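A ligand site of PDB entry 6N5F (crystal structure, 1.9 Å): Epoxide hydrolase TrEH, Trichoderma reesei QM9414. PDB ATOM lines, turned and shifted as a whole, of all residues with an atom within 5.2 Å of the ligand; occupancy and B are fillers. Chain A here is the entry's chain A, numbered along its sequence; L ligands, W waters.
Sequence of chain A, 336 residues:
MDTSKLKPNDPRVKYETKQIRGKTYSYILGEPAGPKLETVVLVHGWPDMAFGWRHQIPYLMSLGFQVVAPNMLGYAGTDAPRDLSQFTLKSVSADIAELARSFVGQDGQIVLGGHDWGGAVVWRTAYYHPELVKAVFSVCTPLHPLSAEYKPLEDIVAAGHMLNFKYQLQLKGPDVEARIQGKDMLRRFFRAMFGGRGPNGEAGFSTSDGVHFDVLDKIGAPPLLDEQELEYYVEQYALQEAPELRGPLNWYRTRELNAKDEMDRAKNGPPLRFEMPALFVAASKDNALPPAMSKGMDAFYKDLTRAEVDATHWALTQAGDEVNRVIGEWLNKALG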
ATOM      1  N   TRP A  46     -11.749  12.207  23.083  1.00  0.00           N
ATOM      2  CA  TRP A  46     -12.013  11.097  22.139  1.00  0.00           C
ATOM      3  C   TRP A  46     -13.491  10.676  22.179  1.00  0.00           C
ATOM      4  O   TRP A  46     -14.065  10.584  23.265  1.00  0.00           O
ATOM      5  CB  TRP A  46     -11.120   9.882  22.485  1.00  0.00           C
ATOM      6  CG  TRP A  46     -11.215   8.721  21.463  1.00  0.00           C
ATOM      7  CD1 TRP A  46     -10.383   8.484  20.400  1.00  0.00           C
ATOM      8  CD2 TRP A  46     -12.193   7.659  21.449  1.00  0.00           C
ATOM      9  NE1 TRP A  46     -10.793   7.345  19.695  1.00  0.00           N
ATOM     10  CE2 TRP A  46     -11.896   6.829  20.338  1.00  0.00           C
ATOM     11  CE3 TRP A  46     -13.293   7.347  22.257  1.00  0.00           C
ATOM     12  CZ2 TRP A  46     -12.674   5.704  20.024  1.00  0.00           C
ATOM     13  CZ3 TRP A  46     -14.050   6.233  21.952  1.00  0.00           C
ATOM     14  CH2 TRP A  46     -13.742   5.419  20.830  1.00  0.00           C
ATOM     15  N   PRO A  47     -14.134  10.461  21.007  1.00  0.00           N
ATOM     16  CA  PRO A  47     -13.713  10.717  19.626  1.00  0.00           C
ATOM     17  C   PRO A  47     -14.382  11.990  19.206  1.00  0.00           C
ATOM     18  O   PRO A  47     -15.462  11.959  18.595  1.00  0.00           O
ATOM     19  CB  PRO A  47     -14.249   9.491  18.840  1.00  0.00           C
ATOM     20  CG  PRO A  47     -15.444   8.955  19.708  1.00  0.00           C
ATOM     21  CD  PRO A  47     -15.450   9.787  21.014  1.00  0.00           C
ATOM     22  N   ASP A 116     -12.731  15.461  28.639  1.00  0.00           N
ATOM     23  CA  ASP A 116     -12.346  14.074  28.286  1.00  0.00           C
ATOM     24  C   ASP A 116     -10.821  14.023  28.303  1.00  0.00           C
ATOM     25  O   ASP A 116     -10.231  14.521  29.262  1.00  0.00           O
ATOM     26  CB  ASP A 116     -13.000  13.661  26.978  1.00  0.00           C
ATOM     27  CG  ASP A 116     -12.797  12.186  26.707  1.00  0.00           C
ATOM     28  OD1 ASP A 116     -13.475  11.369  27.363  1.00  0.00           O
ATOM     29  OD2 ASP A 116     -11.913  11.853  25.874  1.00  0.00           O
ATOM     30  N   TRP A 117     -10.156  13.392  27.307  1.00  0.00           N
ATOM     31  CA  TRP A 117      -8.686  13.404  27.306  1.00  0.00           C
ATOM     32  C   TRP A 117      -8.136  14.810  27.367  1.00  0.00           C
ATOM     33  O   TRP A 117      -7.061  15.027  27.934  1.00  0.00           O
ATOM     34  CB  TRP A 117      -8.090  12.673  26.066  1.00  0.00           C
ATOM     35  CG  TRP A 117      -7.952  11.149  26.241  1.00  0.00           C
ATOM     36  CD1 TRP A 117      -8.537  10.166  25.462  1.00  0.00           C
ATOM     37  CD2 TRP A 117      -7.175  10.460  27.234  1.00  0.00           C
ATOM     38  NE1 TRP A 117      -8.178   8.920  25.919  1.00  0.00           N
ATOM     39  CE2 TRP A 117      -7.342   9.066  27.002  1.00  0.00           C
ATOM     40  CE3 TRP A 117      -6.356  10.876  28.302  1.00  0.00           C
ATOM     41  CZ2 TRP A 117      -6.758   8.098  27.811  1.00  0.00           C
ATOM     42  CZ3 TRP A 117      -5.759   9.910  29.100  1.00  0.00           C
ATOM     43  CH2 TRP A 117      -5.959   8.539  28.850  1.00  0.00           C
ATOM     44  N   ALA A 120      -7.650  15.751  30.997  1.00  0.00           N
ATOM     45  CA  ALA A 120      -6.349  15.273  31.466  1.00  0.00           C
ATOM     46  C   ALA A 120      -5.212  16.141  30.934  1.00  0.00           C
ATOM     47  O   ALA A 120      -4.263  16.431  31.667  1.00  0.00           O
ATOM     48  CB  ALA A 120      -6.133  13.807  31.073  1.00  0.00           C
ATOM     49  N   THR A 141     -13.502  15.270  33.303  1.00  0.00           N
ATOM     50  CA  THR A 141     -12.265  14.572  33.660  1.00  0.00           C
ATOM     51  C   THR A 141     -11.705  15.112  34.960  1.00  0.00           C
ATOM     52  O   THR A 141     -11.348  16.299  35.026  1.00  0.00           O
ATOM     53  CB  THR A 141     -11.237  14.733  32.548  1.00  0.00           C
ATOM     54  OG1 THR A 141     -11.902  14.456  31.309  1.00  0.00           O
ATOM     55  CG2 THR A 141     -10.061  13.786  32.743  1.00  0.00           C
ATOM     56  N   PRO A 142     -11.644  14.310  36.026  1.00  0.00           N
ATOM     57  CA  PRO A 142     -11.033  14.786  37.264  1.00  0.00           C
ATOM     58  C   PRO A 142      -9.511  14.705  37.152  1.00  0.00           C
ATOM     59  O   PRO A 142      -8.949  14.186  36.180  1.00  0.00           O
ATOM     60  CB  PRO A 142     -11.574  13.796  38.306  1.00  0.00           C
ATOM     61  CG  PRO A 142     -11.583  12.516  37.552  1.00  0.00           C
ATOM     62  CD  PRO A 142     -12.002  12.888  36.125  1.00  0.00           C
ATOM     63  N   LEU A 143      -8.852  15.243  38.166  1.00  0.00           N
ATOM     64  CA  LEU A 143      -7.401  15.066  38.270  1.00  0.00           C
ATOM     65  C   LEU A 143      -7.061  13.614  38.562  1.00  0.00           C
ATOM     66  O   LEU A 143      -7.785  12.919  39.277  1.00  0.00           O
ATOM     67  CB  LEU A 143      -6.849  15.969  39.382  1.00  0.00           C
ATOM     68  CG  LEU A 143      -5.333  15.998  39.589  1.00  0.00           C
ATOM     69  CD1 LEU A 143      -4.667  16.656  38.386  1.00  0.00           C
ATOM     70  CD2 LEU A 143      -4.972  16.776  40.865  1.00  0.00           C
ATOM     71  N   HIS A 144      -5.930  13.146  38.018  1.00  0.00           N
ATOM     72  CA  HIS A 144      -5.408  11.870  38.467  1.00  0.00           C
ATOM     73  C   HIS A 144      -3.996  12.100  38.965  1.00  0.00           C
ATOM     74  O   HIS A 144      -3.300  13.000  38.477  1.00  0.00           O
ATOM     75  CB  HIS A 144      -5.425  10.771  37.368  1.00  0.00           C
ATOM     76  CG  HIS A 144      -4.523  11.018  36.191  1.00  0.00           C
ATOM     77  ND1 HIS A 144      -4.714  12.058  35.309  1.00  0.00           N
ATOM     78  CD2 HIS A 144      -3.468  10.301  35.717  1.00  0.00           C
ATOM     79  CE1 HIS A 144      -3.777  12.012  34.367  1.00  0.00           C
ATOM     80  NE2 HIS A 144      -3.017  10.945  34.587  1.00  0.00           N
ATOM     81  N   PHE A 165     -12.762   1.592  32.896  1.00  0.00           N
ATOM     82  CA  PHE A 165     -11.833   1.873  31.797  1.00  0.00           C
ATOM     83  C   PHE A 165     -11.523   0.631  30.945  1.00  0.00           C
ATOM     84  O   PHE A 165     -10.629   0.693  30.083  1.00  0.00           O
ATOM     85  CB  PHE A 165     -10.494   2.428  32.333  1.00  0.00           C
ATOM     86  CG  PHE A 165     -10.598   3.836  32.890  1.00  0.00           C
ATOM     87  CD1 PHE A 165     -11.280   4.832  32.206  1.00  0.00           C
ATOM     88  CD2 PHE A 165     -10.026   4.155  34.114  1.00  0.00           C
ATOM     89  CE1 PHE A 165     -11.375   6.134  32.725  1.00  0.00           C
ATOM     90  CE2 PHE A 165     -10.113   5.452  34.643  1.00  0.00           C
ATOM     91  CZ  PHE A 165     -10.782   6.449  33.928  1.00  0.00           C
ATOM     92  N   TYR A 167     -12.883  -0.724  28.494  1.00  0.00           N
ATOM     93  CA  TYR A 167     -13.015  -0.483  27.053  1.00  0.00           C
ATOM     94  C   TYR A 167     -11.714   0.016  26.430  1.00  0.00           C
ATOM     95  O   TYR A 167     -11.530  -0.139  25.211  1.00  0.00           O
ATOM     96  CB  TYR A 167     -14.120   0.568  26.782  1.00  0.00           C
ATOM     97  CG  TYR A 167     -13.709   1.962  27.261  1.00  0.00           C
ATOM     98  CD1 TYR A 167     -13.937   2.362  28.568  1.00  0.00           C
ATOM     99  CD2 TYR A 167     -13.039   2.848  26.414  1.00  0.00           C
ATOM    100  CE1 TYR A 167     -13.542   3.596  29.041  1.00  0.00           C
ATOM    101  CE2 TYR A 167     -12.618   4.136  26.875  1.00  0.00           C
ATOM    102  CZ  TYR A 167     -12.879   4.487  28.194  1.00  0.00           C
ATOM    103  OH  TYR A 167     -12.489   5.713  28.688  1.00  0.00           O
ATOM    104  N   GLN A 168     -10.802   0.596  27.229  1.00  0.00           N
ATOM    105  CA  GLN A 168      -9.534   1.061  26.669  1.00  0.00           C
ATOM    106  C   GLN A 168      -8.676  -0.083  26.144  1.00  0.00           C
ATOM    107  O   GLN A 168      -7.788   0.158  25.319  1.00  0.00           O
ATOM    108  CB  GLN A 168      -8.762   1.878  27.721  1.00  0.00           C
ATOM    109  CG  GLN A 168      -9.507   3.135  28.177  1.00  0.00           C
ATOM    110  CD  GLN A 168      -8.674   4.046  29.073  1.00  0.00           C
ATOM    111  OE1 GLN A 168      -7.522   3.749  29.366  1.00  0.00           O
ATOM    112  NE2 GLN A 168      -9.264   5.142  29.504  1.00  0.00           N
ATOM    113  N   ALA A 192     -23.276   5.613  16.815  1.00  0.00           N
ATOM    114  CA  ALA A 192     -23.130   4.834  18.045  1.00  0.00           C
ATOM    115  C   ALA A 192     -22.582   5.692  19.189  1.00  0.00           C
ATOM    116  O   ALA A 192     -23.170   5.720  20.273  1.00  0.00           O
ATOM    117  CB  ALA A 192     -22.212   3.638  17.779  1.00  0.00           C
ATOM    118  N   MET A 193     -21.487   6.398  18.954  1.00  0.00           N
ATOM    119  CA  MET A 193     -20.832   7.117  20.044  1.00  0.00           C
ATOM    120  C   MET A 193     -21.691   8.261  20.569  1.00  0.00           C
ATOM    121  O   MET A 193     -21.534   8.674  21.724  1.00  0.00           O
ATOM    122  CB  MET A 193     -19.469   7.643  19.577  1.00  0.00           C
ATOM    123  CG  MET A 193     -18.489   6.541  19.156  1.00  0.00           C
ATOM    124  SD  MET A 193     -18.207   5.262  20.429  1.00  0.00           S
ATOM    125  CE  MET A 193     -17.442   6.281  21.688  1.00  0.00           C
ATOM    126  N   PHE A 194     -22.599   8.809  19.756  1.00  0.00           N
ATOM    127  CA  PHE A 194     -23.463   9.880  20.222  1.00  0.00           C
ATOM    128  C   PHE A 194     -24.881   9.407  20.521  1.00  0.00           C
ATOM    129  O   PHE A 194     -25.834  10.193  20.487  1.00  0.00           O
ATOM    130  CB  PHE A 194     -23.410  11.061  19.243  1.00  0.00           C
ATOM    131  CG  PHE A 194     -22.081  11.803  19.295  1.00  0.00           C
ATOM    132  CD1 PHE A 194     -21.002  11.359  18.543  1.00  0.00           C
ATOM    133  CD2 PHE A 194     -21.896  12.876  20.144  1.00  0.00           C
ATOM    134  CE1 PHE A 194     -19.738  12.025  18.609  1.00  0.00           C
ATOM    135  CE2 PHE A 194     -20.654  13.546  20.221  1.00  0.00           C
ATOM    136  CZ  PHE A 194     -19.593  13.114  19.440  1.00  0.00           C
ATOM    137  N   GLY A 195     -25.025   8.118  20.856  1.00  0.00           N
ATOM    138  CA  GLY A 195     -26.205   7.647  21.562  1.00  0.00           C
ATOM    139  C   GLY A 195     -27.279   6.997  20.734  1.00  0.00           C
ATOM    140  O   GLY A 195     -28.372   6.761  21.250  1.00  0.00           O
ATOM    141  N   PHE A 205     -21.743   1.286  22.200  1.00  0.00           N
ATOM    142  CA  PHE A 205     -20.534   1.421  23.002  1.00  0.00           C
ATOM    143  C   PHE A 205     -20.852   1.046  24.449  1.00  0.00           C
ATOM    144  O   PHE A 205     -21.926   1.373  24.953  1.00  0.00           O
ATOM    145  CB  PHE A 205     -19.983   2.868  22.941  1.00  0.00           C
ATOM    146  CG  PHE A 205     -18.742   3.081  23.780  1.00  0.00           C
ATOM    147  CD1 PHE A 205     -17.496   2.876  23.244  1.00  0.00           C
ATOM    148  CD2 PHE A 205     -18.840   3.488  25.099  1.00  0.00           C
ATOM    149  CE1 PHE A 205     -16.351   3.078  23.998  1.00  0.00           C
ATOM    150  CE2 PHE A 205     -17.702   3.696  25.873  1.00  0.00           C
ATOM    151  CZ  PHE A 205     -16.480   3.495  25.319  1.00  0.00           C
ATOM    152  N   TYR A 252      -4.771   5.910  23.459  1.00  0.00           N
ATOM    153  CA  TYR A 252      -4.885   4.768  24.361  1.00  0.00           C
ATOM    154  C   TYR A 252      -3.620   3.920  24.399  1.00  0.00           C
ATOM    155  O   TYR A 252      -3.581   2.917  25.119  1.00  0.00           O
ATOM    156  CB  TYR A 252      -6.079   3.909  23.944  1.00  0.00           C
ATOM    157  CG  TYR A 252      -7.330   4.732  24.086  1.00  0.00           C
ATOM    158  CD1 TYR A 252      -7.912   4.913  25.327  1.00  0.00           C
ATOM    159  CD2 TYR A 252      -7.849   5.427  22.988  1.00  0.00           C
ATOM    160  CE1 TYR A 252      -8.995   5.729  25.490  1.00  0.00           C
ATOM    161  CE2 TYR A 252      -8.963   6.252  23.143  1.00  0.00           C
ATOM    162  CZ  TYR A 252      -9.524   6.394  24.393  1.00  0.00           C
ATOM    163  OH  TYR A 252     -10.633   7.206  24.588  1.00  0.00           O
ATOM    164  N   ALA A 288     -17.918   6.477  31.998  1.00  0.00           N
ATOM    165  CA  ALA A 288     -16.472   6.375  31.870  1.00  0.00           C
ATOM    166  C   ALA A 288     -15.753   7.240  32.884  1.00  0.00           C
ATOM    167  O   ALA A 288     -14.700   6.843  33.405  1.00  0.00           O
ATOM    168  CB  ALA A 288     -16.053   6.767  30.456  1.00  0.00           C
ATOM    169  N   LEU A 289     -16.284   8.445  33.169  1.00  0.00           N
ATOM    170  CA  LEU A 289     -15.665   9.399  34.086  1.00  0.00           C
ATOM    171  C   LEU A 289     -16.684   9.805  35.146  1.00  0.00           C
ATOM    172  O   LEU A 289     -17.205  10.937  35.141  1.00  0.00           O
ATOM    173  CB  LEU A 289     -15.139  10.626  33.340  1.00  0.00           C
ATOM    174  CG  LEU A 289     -14.086  10.268  32.268  1.00  0.00           C
ATOM    175  CD1 LEU A 289     -13.965  11.461  31.275  1.00  0.00           C
ATOM    176  CD2 LEU A 289     -12.753   9.949  32.902  1.00  0.00           C
ATOM    177  N   MET A 293     -15.286   9.541  40.934  1.00  0.00           N
ATOM    178  CA  MET A 293     -13.864   9.413  40.698  1.00  0.00           C
ATOM    179  C   MET A 293     -13.088  10.668  41.120  1.00  0.00           C
ATOM    180  O   MET A 293     -11.873  10.603  41.305  1.00  0.00           O
ATOM    181  CB  MET A 293     -13.612   9.109  39.218  1.00  0.00           C
ATOM    182  CG  MET A 293     -12.277   8.499  38.926  1.00  0.00           C
ATOM    183  SD  MET A 293     -12.262   7.715  37.299  1.00  0.00           S
ATOM    184  CE  MET A 293     -13.152   8.917  36.352  1.00  0.00           C
ATOM    185  N   THR A 312     -24.982  13.303  30.202  1.00  0.00           N
ATOM    186  CA  THR A 312     -24.124  12.202  29.797  1.00  0.00           C
ATOM    187  C   THR A 312     -22.694  12.700  29.648  1.00  0.00           C
ATOM    188  O   THR A 312     -22.374  13.876  29.906  1.00  0.00           O
ATOM    189  CB  THR A 312     -24.582  11.600  28.463  1.00  0.00           C
ATOM    190  OG1 THR A 312     -24.472  12.589  27.424  1.00  0.00           O
ATOM    191  CG2 THR A 312     -26.013  11.087  28.553  1.00  0.00           C
ATOM    192  N   HIS A 313     -21.834  11.814  29.158  1.00  0.00           N
ATOM    193  CA  HIS A 313     -20.482  12.196  28.805  1.00  0.00           C
ATOM    194  C   HIS A 313     -20.439  13.412  27.885  1.00  0.00           C
ATOM    195  O   HIS A 313     -19.499  14.210  27.957  1.00  0.00           O
ATOM    196  CB  HIS A 313     -19.758  11.027  28.138  1.00  0.00           C
ATOM    197  CG  HIS A 313     -18.386  11.375  27.664  1.00  0.00           C
ATOM    198  ND1 HIS A 313     -17.323  11.507  28.524  1.00  0.00           N
ATOM    199  CD2 HIS A 313     -17.916  11.692  26.429  1.00  0.00           C
ATOM    200  CE1 HIS A 313     -16.246  11.868  27.846  1.00  0.00           C
ATOM    201  NE2 HIS A 313     -16.584  11.983  26.570  1.00  0.00           N
ATOM    202  N   TRP A 314     -21.424  13.580  27.005  1.00  0.00           N
ATOM    203  CA  TRP A 314     -21.387  14.687  26.048  1.00  0.00           C
ATOM    204  C   TRP A 314     -21.980  15.977  26.615  1.00  0.00           C
ATOM    205  O   TRP A 314     -22.867  16.610  26.030  1.00  0.00           O
ATOM    206  CB  TRP A 314     -22.078  14.290  24.752  1.00  0.00           C
ATOM    207  CG  TRP A 314     -21.408  13.112  24.109  1.00  0.00           C
ATOM    208  CD1 TRP A 314     -21.938  11.865  23.873  1.00  0.00           C
ATOM    209  CD2 TRP A 314     -20.061  13.083  23.604  1.00  0.00           C
ATOM    210  NE1 TRP A 314     -20.990  11.057  23.267  1.00  0.00           N
ATOM    211  CE2 TRP A 314     -19.829  11.782  23.087  1.00  0.00           C
ATOM    212  CE3 TRP A 314     -19.023  14.025  23.547  1.00  0.00           C
ATOM    213  CZ2 TRP A 314     -18.622  11.405  22.508  1.00  0.00           C
ATOM    214  CZ3 TRP A 314     -17.802  13.651  22.976  1.00  0.00           C
ATOM    215  CH2 TRP A 314     -17.614  12.357  22.462  1.00  0.00           C
HETATM  216  C1  LIG L   1     -15.094   7.867  26.584  1.00  0.00           C
HETATM  217  C2  LIG L   1     -17.366   8.185  25.250  1.00  0.00           C
HETATM  218  C3  LIG L   1     -19.734   7.529  24.142  1.00  0.00           C
HETATM  219  C4  LIG L   1      -8.765  10.403  35.086  1.00  0.00           C
HETATM  220  C5  LIG L   1      -7.730   9.424  34.489  1.00  0.00           C
HETATM  221  C6  LIG L   1      -7.019  10.075  33.304  1.00  0.00           C
HETATM  222  C7  LIG L   1      -8.036  10.551  32.268  1.00  0.00           C
HETATM  223  C8  LIG L   1      -8.746   9.391  31.540  1.00  0.00           C
HETATM  224  C9  LIG L   1      -9.660   9.962  30.447  1.00  0.00           C
HETATM  225  C10 LIG L   1     -10.294   8.863  29.583  1.00  0.00           C
HETATM  226  C11 LIG L   1     -10.903   9.527  28.351  1.00  0.00           C
HETATM  227  C12 LIG L   1     -11.651   8.545  27.471  1.00  0.00           C
HETATM  228  O1  LIG L   1     -11.223   7.431  27.280  1.00  0.00           O
HETATM  229  N1  LIG L   1     -12.894   8.988  26.889  1.00  0.00           N
HETATM  230  C13 LIG L   1     -13.692   8.090  26.021  1.00  0.00           C
HETATM  231  C14 LIG L   1     -16.115   7.303  25.560  1.00  0.00           C
HETATM  232  C15 LIG L   1     -18.746   7.451  25.342  1.00  0.00           C
HETATM  233  C16 LIG L   1     -21.158   6.902  24.284  1.00  0.00           C
HETATM  234  C17 LIG L   1     -22.175   7.906  24.871  1.00  0.00           C
HETATM  235  N2  LIG L   1     -21.720   8.635  26.022  1.00  0.00           N
HETATM  236  O2  LIG L   1     -23.304   8.105  24.448  1.00  0.00           O
HETATM  237  O   HOH W   1     -22.536   8.943  29.287  1.00  0.00           O
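Water W1 bridges the backbone NH (N) of His 313 and a nitrogen (N2) of the ligand.
O2 of the ligand lies close to O of Met 193 (3.3 Å). Residues that only touch the ligand: Trp 46, Trp 117, Ala 120, Thr 141, Pro 142, His 144, Gln 168, Gly 195, Phe 205, Leu 289, His 313 and Trp 314. Hydrophobic or aromatic side chains that line the ligand: Trp 46, Trp 117, Ala 120, His 144, Tyr 167, Met 193, Phe 205, Tyr 252, Leu 289, His 313 and Trp 314. Within 4 Å of the ligand: Trp 46, Asp 116, Trp 117, Ala 120, Thr 141, Pro 142, His 144, Tyr 167, Gln 168, Met 193, Gly 195, Phe 205, Tyr 252, Leu 289, His 313 and Trp 314.
The side-chain hydroxyl (OH) of Tyr 167 is in hydrogen-bond range of the side-chain amide nitrogen (NE2) of Gln 168, 3.4 Å away. The backbone NH (N) of Trp 46 is in hydrogen-bond range of the side-chain carboxylate (OD2) of Asp 116, at 2.8 Å. OD1 of Asp 116 sits close to NE2 of His 313, at 3.3 Å. OG1 of Thr 141 lies within hydrogen-bond range of O of Asp 116 (2.6 Å). OH of Tyr 252 lies close to NE1 of Trp 117 (3.3 Å). The indole nitrogen of Trp 314 is in hydrogen-bond range of the backbone carbonyl oxygen of Met 193 (2.9 Å). OG1 of Thr 312 lies close to N of Trp 314 (3.2 Å).
OD1 of Asp 116 is in hydrogen-bond range of N1 of the ligand, at 2.5 Å. The side-chain hydroxyl (OH) of Tyr 252 is in hydrogen-bond range of an oxygen (O1) of the ligand. O1 of the ligand sits at hydrogen-bond distance from OH of Tyr 167 (2.6 Å).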
